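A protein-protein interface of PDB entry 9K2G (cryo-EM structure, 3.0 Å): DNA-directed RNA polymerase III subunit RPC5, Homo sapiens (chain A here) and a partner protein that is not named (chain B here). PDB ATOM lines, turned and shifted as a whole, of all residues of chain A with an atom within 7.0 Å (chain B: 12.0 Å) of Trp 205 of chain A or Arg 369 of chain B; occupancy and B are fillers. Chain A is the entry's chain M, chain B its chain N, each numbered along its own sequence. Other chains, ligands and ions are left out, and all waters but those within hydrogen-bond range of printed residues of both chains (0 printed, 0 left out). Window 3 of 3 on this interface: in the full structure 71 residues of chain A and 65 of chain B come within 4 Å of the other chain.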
ATOM      1  N   ALA A  47       5.925 -22.297  18.856  1.00  0.00           N
ATOM      2  CA  ALA A  47       6.875 -21.200  19.014  1.00  0.00           C
ATOM      3  C   ALA A  47       6.801 -20.293  17.798  1.00  0.00           C
ATOM      4  O   ALA A  47       7.209 -20.684  16.705  1.00  0.00           O
ATOM      5  CB  ALA A  47       8.294 -21.719  19.212  1.00  0.00           C
ATOM      6  N   LYS A  48       6.294 -19.079  17.984  1.00  0.00           N
ATOM      7  CA  LYS A  48       6.347 -18.079  16.934  1.00  0.00           C
ATOM      8  C   LYS A  48       7.675 -17.339  17.006  1.00  0.00           C
ATOM      9  O   LYS A  48       8.249 -17.178  18.082  1.00  0.00           O
ATOM     10  CB  LYS A  48       5.176 -17.101  17.069  1.00  0.00           C
ATOM     11  CG  LYS A  48       3.829 -17.785  17.228  1.00  0.00           C
ATOM     12  CD  LYS A  48       2.724 -16.772  17.425  1.00  0.00           C
ATOM     13  CE  LYS A  48       2.599 -15.850  16.223  1.00  0.00           C
ATOM     14  NZ  LYS A  48       1.682 -14.707  16.481  1.00  0.00           N
ATOM     15  N   ILE A  49       8.180 -16.915  15.851  1.00  0.00           N
ATOM     16  CA  ILE A  49       9.465 -16.229  15.805  1.00  0.00           C
ATOM     17  C   ILE A  49       9.539 -15.366  14.556  1.00  0.00           C
ATOM     18  O   ILE A  49       8.912 -15.662  13.536  1.00  0.00           O
ATOM     19  CB  ILE A  49      10.649 -17.227  15.864  1.00  0.00           C
ATOM     20  CG1 ILE A  49      11.924 -16.516  16.333  1.00  0.00           C
ATOM     21  CG2 ILE A  49      10.874 -17.881  14.510  1.00  0.00           C
ATOM     22  CD1 ILE A  49      13.093 -17.447  16.549  1.00  0.00           C
ATOM     23  N   LYS A  50      10.303 -14.281  14.648  1.00  0.00           N
ATOM     24  CA  LYS A  50      10.606 -13.433  13.512  1.00  0.00           C
ATOM     25  C   LYS A  50      12.097 -13.512  13.220  1.00  0.00           C
ATOM     26  O   LYS A  50      12.904 -13.233  14.120  1.00  0.00           O
ATOM     27  CB  LYS A  50      10.190 -11.987  13.784  1.00  0.00           C
ATOM     28  CG  LYS A  50       8.735 -11.839  14.206  1.00  0.00           C
ATOM     29  CD  LYS A  50       8.218 -10.437  13.939  1.00  0.00           C
ATOM     30  CE  LYS A  50       6.710 -10.376  14.104  1.00  0.00           C
ATOM     31  NZ  LYS A  50       6.126  -9.154  13.490  1.00  0.00           N
ATOM     32  N   PRO A  51      12.507 -13.907  12.012  1.00  0.00           N
ATOM     33  CA  PRO A  51      13.955 -14.008  11.739  1.00  0.00           C
ATOM     34  C   PRO A  51      14.686 -12.692  11.934  1.00  0.00           C
ATOM     35  O   PRO A  51      15.673 -12.636  12.680  1.00  0.00           O
ATOM     36  CB  PRO A  51      13.997 -14.498  10.283  1.00  0.00           C
ATOM     37  CG  PRO A  51      12.670 -14.114   9.706  1.00  0.00           C
ATOM     38  CD  PRO A  51      11.690 -14.238  10.833  1.00  0.00           C
ATOM     39  N   LYS A  55      12.141 -11.960  17.834  1.00  0.00           N
ATOM     40  CA  LYS A  55      11.223 -11.885  18.963  1.00  0.00           C
ATOM     41  C   LYS A  55      10.459 -13.208  19.007  1.00  0.00           C
ATOM     42  O   LYS A  55       9.480 -13.381  18.280  1.00  0.00           O
ATOM     43  CB  LYS A  55      10.283 -10.696  18.834  1.00  0.00           C
ATOM     44  CG  LYS A  55       9.338 -10.507  20.013  1.00  0.00           C
ATOM     45  CD  LYS A  55       8.688  -9.129  19.990  1.00  0.00           C
ATOM     46  CE  LYS A  55       7.590  -9.033  18.941  1.00  0.00           C
ATOM     47  NZ  LYS A  55       6.338  -9.708  19.386  1.00  0.00           N
ATOM     48  N   VAL A  56      10.914 -14.125  19.851  1.00  0.00           N
ATOM     49  CA  VAL A  56      10.316 -15.458  19.937  1.00  0.00           C
ATOM     50  C   VAL A  56       9.245 -15.462  21.015  1.00  0.00           C
ATOM     51  O   VAL A  56       9.412 -14.895  22.100  1.00  0.00           O
ATOM     52  CB  VAL A  56      11.392 -16.533  20.197  1.00  0.00           C
ATOM     53  CG1 VAL A  56      12.077 -16.330  21.542  1.00  0.00           C
ATOM     54  CG2 VAL A  56      10.787 -17.929  20.106  1.00  0.00           C
ATOM     55  N   GLU A  57       8.112 -16.082  20.698  1.00  0.00           N
ATOM     56  CA  GLU A  57       6.996 -16.243  21.622  1.00  0.00           C
ATOM     57  C   GLU A  57       6.719 -17.736  21.769  1.00  0.00           C
ATOM     58  O   GLU A  57       6.281 -18.388  20.814  1.00  0.00           O
ATOM     59  CB  GLU A  57       5.758 -15.495  21.128  1.00  0.00           C
ATOM     60  CG  GLU A  57       4.549 -15.626  22.037  1.00  0.00           C
ATOM     61  CD  GLU A  57       3.515 -14.543  21.788  1.00  0.00           C
ATOM     62  OE1 GLU A  57       3.831 -13.582  21.057  1.00  0.00           O
ATOM     63  OE2 GLU A  57       2.396 -14.657  22.321  1.00  0.00           O
ATOM     64  N   CYS A 103       7.001 -14.307  26.164  1.00  0.00           N
ATOM     65  CA  CYS A 103       7.462 -13.352  25.168  1.00  0.00           C
ATOM     66  C   CYS A 103       8.926 -13.023  25.402  1.00  0.00           C
ATOM     67  O   CYS A 103       9.407 -13.004  26.539  1.00  0.00           O
ATOM     68  CB  CYS A 103       6.626 -12.065  25.205  1.00  0.00           C
ATOM     69  SG  CYS A 103       7.064 -10.867  23.929  1.00  0.00           S
ATOM     70  N   SER A 104       9.642 -12.760  24.313  1.00  0.00           N
ATOM     71  CA  SER A 104      11.072 -12.504  24.366  1.00  0.00           C
ATOM     72  C   SER A 104      11.368 -11.015  24.253  1.00  0.00           C
ATOM     73  O   SER A 104      10.729 -10.298  23.473  1.00  0.00           O
ATOM     74  CB  SER A 104      11.810 -13.250  23.257  1.00  0.00           C
ATOM     75  OG  SER A 104      11.396 -12.803  21.980  1.00  0.00           O
ATOM     76  N   HIS A 200       7.241  -3.428  13.429  1.00  0.00           N
ATOM     77  CA  HIS A 200       7.579  -4.769  13.902  1.00  0.00           C
ATOM     78  C   HIS A 200       6.524  -5.784  13.477  1.00  0.00           C
ATOM     79  O   HIS A 200       6.859  -6.894  13.042  1.00  0.00           O
ATOM     80  CB  HIS A 200       7.737  -4.773  15.421  1.00  0.00           C
ATOM     81  CG  HIS A 200       8.994  -4.118  15.906  1.00  0.00           C
ATOM     82  ND1 HIS A 200      10.249  -4.559  15.547  1.00  0.00           N
ATOM     83  CD2 HIS A 200       9.189  -3.063  16.727  1.00  0.00           C
ATOM     84  CE1 HIS A 200      11.161  -3.800  16.124  1.00  0.00           C
ATOM     85  NE2 HIS A 200      10.546  -2.884  16.845  1.00  0.00           N
ATOM     86  N   ALA A 201       5.241  -5.425  13.601  1.00  0.00           N
ATOM     87  CA  ALA A 201       4.167  -6.334  13.234  1.00  0.00           C
ATOM     88  C   ALA A 201       4.081  -6.571  11.735  1.00  0.00           C
ATOM     89  O   ALA A 201       3.487  -7.573  11.313  1.00  0.00           O
ATOM     90  CB  ALA A 201       2.828  -5.801  13.752  1.00  0.00           C
ATOM     91  N   GLU A 202       4.647  -5.676  10.921  1.00  0.00           N
ATOM     92  CA  GLU A 202       4.613  -5.867   9.474  1.00  0.00           C
ATOM     93  C   GLU A 202       5.358  -7.131   9.050  1.00  0.00           C
ATOM     94  O   GLU A 202       4.985  -7.762   8.056  1.00  0.00           O
ATOM     95  CB  GLU A 202       5.201  -4.646   8.763  1.00  0.00           C
ATOM     96  CG  GLU A 202       4.298  -3.428   8.781  1.00  0.00           C
ATOM     97  CD  GLU A 202       5.003  -2.166   8.316  1.00  0.00           C
ATOM     98  OE1 GLU A 202       6.189  -2.254   7.938  1.00  0.00           O
ATOM     99  OE2 GLU A 202       4.369  -1.088   8.337  1.00  0.00           O
ATOM    100  N   GLU A 203       6.398  -7.510   9.785  1.00  0.00           N
ATOM    101  CA  GLU A 203       7.139  -8.722   9.459  1.00  0.00           C
ATOM    102  C   GLU A 203       6.309  -9.951   9.824  1.00  0.00           C
ATOM    103  O   GLU A 203       5.821 -10.043  10.958  1.00  0.00           O
ATOM    104  CB  GLU A 203       8.477  -8.748  10.186  1.00  0.00           C
ATOM    105  CG  GLU A 203       9.380  -9.908   9.795  1.00  0.00           C
ATOM    106  CD  GLU A 203      10.755  -9.810  10.422  1.00  0.00           C
ATOM    107  OE1 GLU A 203      11.032  -8.793  11.090  1.00  0.00           O
ATOM    108  OE2 GLU A 203      11.561 -10.749  10.252  1.00  0.00           O
ATOM    109  N   PRO A 204       6.132 -10.902   8.913  1.00  0.00           N
ATOM    110  CA  PRO A 204       5.284 -12.062   9.208  1.00  0.00           C
ATOM    111  C   PRO A 204       5.879 -12.961  10.280  1.00  0.00           C
ATOM    112  O   PRO A 204       7.096 -13.050  10.447  1.00  0.00           O
ATOM    113  CB  PRO A 204       5.201 -12.792   7.862  1.00  0.00           C
ATOM    114  CG  PRO A 204       6.450 -12.398   7.150  1.00  0.00           C
ATOM    115  CD  PRO A 204       6.725 -10.978   7.567  1.00  0.00           C
ATOM    116  N   TRP A 205       4.989 -13.633  11.008  1.00  0.00           N
ATOM    117  CA  TRP A 205       5.398 -14.603  12.005  1.00  0.00           C
ATOM    118  C   TRP A 205       5.771 -15.930  11.347  1.00  0.00           C
ATOM    119  O   TRP A 205       5.246 -16.293  10.290  1.00  0.00           O
ATOM    120  CB  TRP A 205       4.293 -14.828  13.031  1.00  0.00           C
ATOM    121  CG  TRP A 205       4.131 -13.713  14.025  1.00  0.00           C
ATOM    122  CD1 TRP A 205       3.171 -12.744  14.022  1.00  0.00           C
ATOM    123  CD2 TRP A 205       4.951 -13.464  15.175  1.00  0.00           C
ATOM    124  NE1 TRP A 205       3.345 -11.905  15.097  1.00  0.00           N
ATOM    125  CE2 TRP A 205       4.429 -12.323  15.817  1.00  0.00           C
ATOM    126  CE3 TRP A 205       6.079 -14.090  15.716  1.00  0.00           C
ATOM    127  CZ2 TRP A 205       4.996 -11.797  16.979  1.00  0.00           C
ATOM    128  CZ3 TRP A 205       6.634 -13.569  16.869  1.00  0.00           C
ATOM    129  CH2 TRP A 205       6.095 -12.434  17.488  1.00  0.00           C
ATOM    130  N   VAL A 206       6.682 -16.652  11.993  1.00  0.00           N
ATOM    131  CA  VAL A 206       7.144 -17.958  11.534  1.00  0.00           C
ATOM    132  C   VAL A 206       6.902 -18.966  12.647  1.00  0.00           C
ATOM    133  O   VAL A 206       7.330 -18.752  13.785  1.00  0.00           O
ATOM    134  CB  VAL A 206       8.631 -17.927  11.133  1.00  0.00           C
ATOM    135  CG1 VAL A 206       9.100 -19.310  10.716  1.00  0.00           C
ATOM    136  CG2 VAL A 206       8.860 -16.925  10.007  1.00  0.00           C
ATOM    137  N   HIS A 207       6.225 -20.066  12.318  1.00  0.00           N
ATOM    138  CA  HIS A 207       5.861 -21.076  13.304  1.00  0.00           C
ATOM    139  C   HIS A 207       6.934 -22.153  13.401  1.00  0.00           C
ATOM    140  O   HIS A 207       7.522 -22.557  12.393  1.00  0.00           O
ATOM    141  CB  HIS A 207       4.515 -21.708  12.955  1.00  0.00           C
ATOM    142  CG  HIS A 207       3.342 -20.821  13.231  1.00  0.00           C
ATOM    143  ND1 HIS A 207       3.016 -19.747  12.432  1.00  0.00           N
ATOM    144  CD2 HIS A 207       2.425 -20.840  14.227  1.00  0.00           C
ATOM    145  CE1 HIS A 207       1.945 -19.146  12.920  1.00  0.00           C
ATOM    146  NE2 HIS A 207       1.567 -19.790  14.010  1.00  0.00           N
ATOM    147  N   LEU A 208       7.176 -22.621  14.626  1.00  0.00           N
ATOM    148  CA  LEU A 208       8.205 -23.605  14.910  1.00  0.00           C
ATOM    149  C   LEU A 208       7.678 -24.627  15.906  1.00  0.00           C
ATOM    150  O   LEU A 208       6.995 -24.275  16.877  1.00  0.00           O
ATOM    151  CB  LEU A 208       9.475 -22.954  15.488  1.00  0.00           C
ATOM    152  CG  LEU A 208      10.127 -21.778  14.765  1.00  0.00           C
ATOM    153  CD1 LEU A 208      11.323 -21.292  15.563  1.00  0.00           C
ATOM    154  CD2 LEU A 208      10.548 -22.167  13.361  1.00  0.00           C
ATOM    155  N   HIS A 209       8.015 -25.889  15.654  1.00  0.00           N
ATOM    156  CA  HIS A 209       7.773 -26.980  16.581  1.00  0.00           C
ATOM    157  C   HIS A 209       8.867 -27.010  17.646  1.00  0.00           C
ATOM    158  O   HIS A 209       9.975 -26.506  17.451  1.00  0.00           O
ATOM    159  CB  HIS A 209       7.728 -28.319  15.844  1.00  0.00           C
ATOM    160  CG  HIS A 209       6.858 -28.310  14.624  1.00  0.00           C
ATOM    161  ND1 HIS A 209       7.374 -28.396  13.346  1.00  0.00           N
ATOM    162  CD2 HIS A 209       5.514 -28.227  14.484  1.00  0.00           C
ATOM    163  CE1 HIS A 209       6.383 -28.367  12.473  1.00  0.00           C
ATOM    164  NE2 HIS A 209       5.245 -28.267  13.137  1.00  0.00           N
ATOM    165  N   VAL B 363      18.028 -23.058  17.189  1.00  0.00           N
ATOM    166  CA  VAL B 363      16.838 -22.751  16.404  1.00  0.00           C
ATOM    167  C   VAL B 363      17.264 -22.819  14.940  1.00  0.00           C
ATOM    168  O   VAL B 363      17.757 -21.844  14.369  1.00  0.00           O
ATOM    169  CB  VAL B 363      16.236 -21.397  16.775  1.00  0.00           C
ATOM    170  CG1 VAL B 363      14.973 -21.136  15.965  1.00  0.00           C
ATOM    171  CG2 VAL B 363      15.936 -21.340  18.271  1.00  0.00           C
ATOM    172  N   GLY B 364      17.077 -23.983  14.329  1.00  0.00           N
ATOM    173  CA  GLY B 364      17.467 -24.176  12.948  1.00  0.00           C
ATOM    174  C   GLY B 364      16.306 -24.103  11.982  1.00  0.00           C
ATOM    175  O   GLY B 364      15.459 -25.002  11.944  1.00  0.00           O
ATOM    176  N   LEU B 365      16.252 -23.029  11.191  1.00  0.00           N
ATOM    177  CA  LEU B 365      15.210 -22.865  10.176  1.00  0.00           C
ATOM    178  C   LEU B 365      15.629 -23.653   8.937  1.00  0.00           C
ATOM    179  O   LEU B 365      16.098 -23.109   7.931  1.00  0.00           O
ATOM    180  CB  LEU B 365      14.984 -21.396   9.852  1.00  0.00           C
ATOM    181  CG  LEU B 365      14.435 -20.496  10.965  1.00  0.00           C
ATOM    182  CD1 LEU B 365      15.559 -19.861  11.779  1.00  0.00           C
ATOM    183  CD2 LEU B 365      13.507 -19.435  10.392  1.00  0.00           C
ATOM    184  N   GLY B 366      15.459 -24.975   9.021  1.00  0.00           N
ATOM    185  CA  GLY B 366      15.783 -25.826   7.887  1.00  0.00           C
ATOM    186  C   GLY B 366      14.942 -25.514   6.669  1.00  0.00           C
ATOM    187  O   GLY B 366      15.422 -25.585   5.537  1.00  0.00           O
ATOM    188  N   ASP B 367      13.675 -25.180   6.886  1.00  0.00           N
ATOM    189  CA  ASP B 367      12.772 -24.770   5.821  1.00  0.00           C
ATOM    190  C   ASP B 367      12.335 -23.331   6.053  1.00  0.00           C
ATOM    191  O   ASP B 367      12.329 -22.827   7.183  1.00  0.00           O
ATOM    192  CB  ASP B 367      11.553 -25.698   5.758  1.00  0.00           C
ATOM    193  CG  ASP B 367      10.692 -25.458   4.528  1.00  0.00           C
ATOM    194  OD1 ASP B 367      11.051 -24.604   3.693  1.00  0.00           O
ATOM    195  OD2 ASP B 367       9.647 -26.133   4.398  1.00  0.00           O
ATOM    196  N   SER B 368      11.966 -22.659   4.961  1.00  0.00           N
ATOM    197  CA  SER B 368      11.465 -21.295   5.050  1.00  0.00           C
ATOM    198  C   SER B 368      10.094 -21.213   5.701  1.00  0.00           C
ATOM    199  O   SER B 368       9.648 -20.104   6.024  1.00  0.00           O
ATOM    200  CB  SER B 368      11.402 -20.669   3.653  1.00  0.00           C
ATOM    201  OG  SER B 368      10.948 -19.323   3.717  1.00  0.00           O
ATOM    202  N   ARG B 369       9.422 -22.351   5.909  1.00  0.00           N
ATOM    203  CA  ARG B 369       8.115 -22.392   6.552  1.00  0.00           C
ATOM    204  C   ARG B 369       8.114 -23.136   7.883  1.00  0.00           C
ATOM    205  O   ARG B 369       7.290 -22.813   8.746  1.00  0.00           O
ATOM    206  CB  ARG B 369       7.084 -23.046   5.615  1.00  0.00           C
ATOM    207  CG  ARG B 369       5.640 -23.036   6.111  1.00  0.00           C
ATOM    208  CD  ARG B 369       5.121 -21.626   6.319  1.00  0.00           C
ATOM    209  NE  ARG B 369       5.356 -21.143   7.675  1.00  0.00           N
ATOM    210  CZ  ARG B 369       5.119 -19.904   8.076  1.00  0.00           C
ATOM    211  NH1 ARG B 369       4.655 -18.985   7.248  1.00  0.00           N
ATOM    212  NH2 ARG B 369       5.360 -19.576   9.342  1.00  0.00           N
ATOM    213  N   THR B 370       9.021 -24.094   8.082  1.00  0.00           N
ATOM    214  CA  THR B 370       9.076 -24.884   9.303  1.00  0.00           C
ATOM    215  C   THR B 370      10.524 -25.000   9.762  1.00  0.00           C
ATOM    216  O   THR B 370      11.418 -25.263   8.947  1.00  0.00           O
ATOM    217  CB  THR B 370       8.471 -26.278   9.081  1.00  0.00           C
ATOM    218  OG1 THR B 370       7.058 -26.158   8.878  1.00  0.00           O
ATOM    219  CG2 THR B 370       8.732 -27.183  10.276  1.00  0.00           C
ATOM    220  N   GLY B 371      10.747 -24.805  11.064  1.00  0.00           N
ATOM    221  CA  GLY B 371      12.073 -24.907  11.629  1.00  0.00           C
ATOM    222  C   GLY B 371      12.074 -25.773  12.880  1.00  0.00           C
ATOM    223  O   GLY B 371      11.018 -26.161  13.394  1.00  0.00           O
ATOM    224  N   GLU B 372      13.278 -26.063  13.361  1.00  0.00           N
ATOM    225  CA  GLU B 372      13.481 -26.921  14.520  1.00  0.00           C
ATOM    226  C   GLU B 372      14.137 -26.136  15.645  1.00  0.00           C
ATOM    227  O   GLU B 372      15.101 -25.401  15.423  1.00  0.00           O
ATOM    228  CB  GLU B 372      14.350 -28.133  14.176  1.00  0.00           C
ATOM    229  CG  GLU B 372      13.738 -29.100  13.183  1.00  0.00           C
ATOM    230  CD  GLU B 372      14.632 -30.293  12.920  1.00  0.00           C
ATOM    231  OE1 GLU B 372      15.755 -30.332  13.473  1.00  0.00           O
ATOM    232  OE2 GLU B 372      14.216 -31.199  12.167  1.00  0.00           O
ATOM    233  N   MET B 373      13.606 -26.301  16.854  1.00  0.00           N
ATOM    234  CA  MET B 373      14.266 -25.844  18.069  1.00  0.00           C
ATOM    235  C   MET B 373      14.857 -27.057  18.769  1.00  0.00           C
ATOM    236  O   MET B 373      14.131 -28.000  19.110  1.00  0.00           O
ATOM    237  CB  MET B 373      13.296 -25.113  18.991  1.00  0.00           C
ATOM    238  CG  MET B 373      12.951 -23.710  18.540  1.00  0.00           C
ATOM    239  SD  MET B 373      11.766 -22.960  19.667  1.00  0.00           S
ATOM    240  CE  MET B 373      10.554 -24.272  19.759  1.00  0.00           C
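O of Ala 47 of chain A sits at hydrogen-bond distance from N of Leu 208 of chain A, 2.8 Å away. The backbone NH (N) of Val 206 of chain A is in hydrogen-bond range of the backbone carbonyl oxygen (O) of Ile 49 of chain A (2.9 Å).
The backbone carbonyl oxygen of Trp 205 of chain A sits at hydrogen-bond distance from the guanidinium group of Arg 369 of chain B, at 3.4 Å. The backbone NH of His 207 of chain A lies close to the guanidinium group of Arg 369 of chain B (3.1 Å).
Printed residues of chain B within 4 Å of Ala 47 of chain A: Met 373 (3.5 Å). No residue of chain B comes within 4 Å of Lys 48 of chain A. No residue of chain B comes within 4 Å of Lys 50 of chain A. No residue of chain B comes within 4 Å of Val 56 of chain A. Ala 201 of chain A touches none of the printed residues of chain B. No residue of chain B comes within 4 Å of Glu 203 of chain A. No residue of chain B comes within 4 Å of Pro 204 of chain A. Of chain B, only Arg 369 (3.4 Å) comes within 4 Å of Trp 205 of chain A. Of chain B, only Arg 369 comes within 4 Å of Val 206 of chain A. Of the printed residues of chain B, Leu 208 of chain A touches Val 363 and Gly 371. Of the printed residues of chain A, Val 363 of chain B touches Leu 208. Gly 366 of chain B touches none of the printed residues of chain A. Arg 369 of chain B touches just these residues of chain A: Trp 205, Val 206 and His 207. Of the printed residues of chain A, Gly 371 of chain B touches Leu 208 (3.5 Å) and His 209 (3.8 Å). The nearest residue of chain A that does not touch Arg 369 of chain B is Leu 208 of chain A (5.7 Å). The nearest printed residue of chain A that does not touch Gly 371 of chain B is His 207 of chain A (4.1 Å).
Of the 20 printed residues of chain A, 6 touch a printed residue of chain B. Printed residues of chain A that touch a printed residue of chain B: Ala 47, Trp 205, Val 206, His 207, Leu 208 and His 209. Hydrophobic or aromatic side chains of chain A within 4 Å of the printed part of chain B: Ala 47, Val 206, His 207, Leu 208 and His 209. Hydrophobic or aromatic side chains of chain B within 4 Å of the printed part of chain A: Val 363 and Met 373. Among the printed residues, 9 pairs touch across the chains.
Ala 47 of chain A touches Met 373 of chain B (CB to CE, 3.5 Å). Val 206 of chain A touches Arg 369 of chain B (CA to NH2, 3.3 Å). Val 363 of chain B touches Leu 208 of chain A (CG1 to CD1, 3.7 Å). N of Gly 371 of chain B touches CD2 of Leu 208 of chain A, 3.5 Å away. CE1 of His 209 of chain A touches CG2 of Thr 370 of chain B, at 3.4 Å. O of Gly 371 of chain B touches N of His 209 of chain A (3.8 Å). His 209 of chain A touches Met 373 of chain B.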
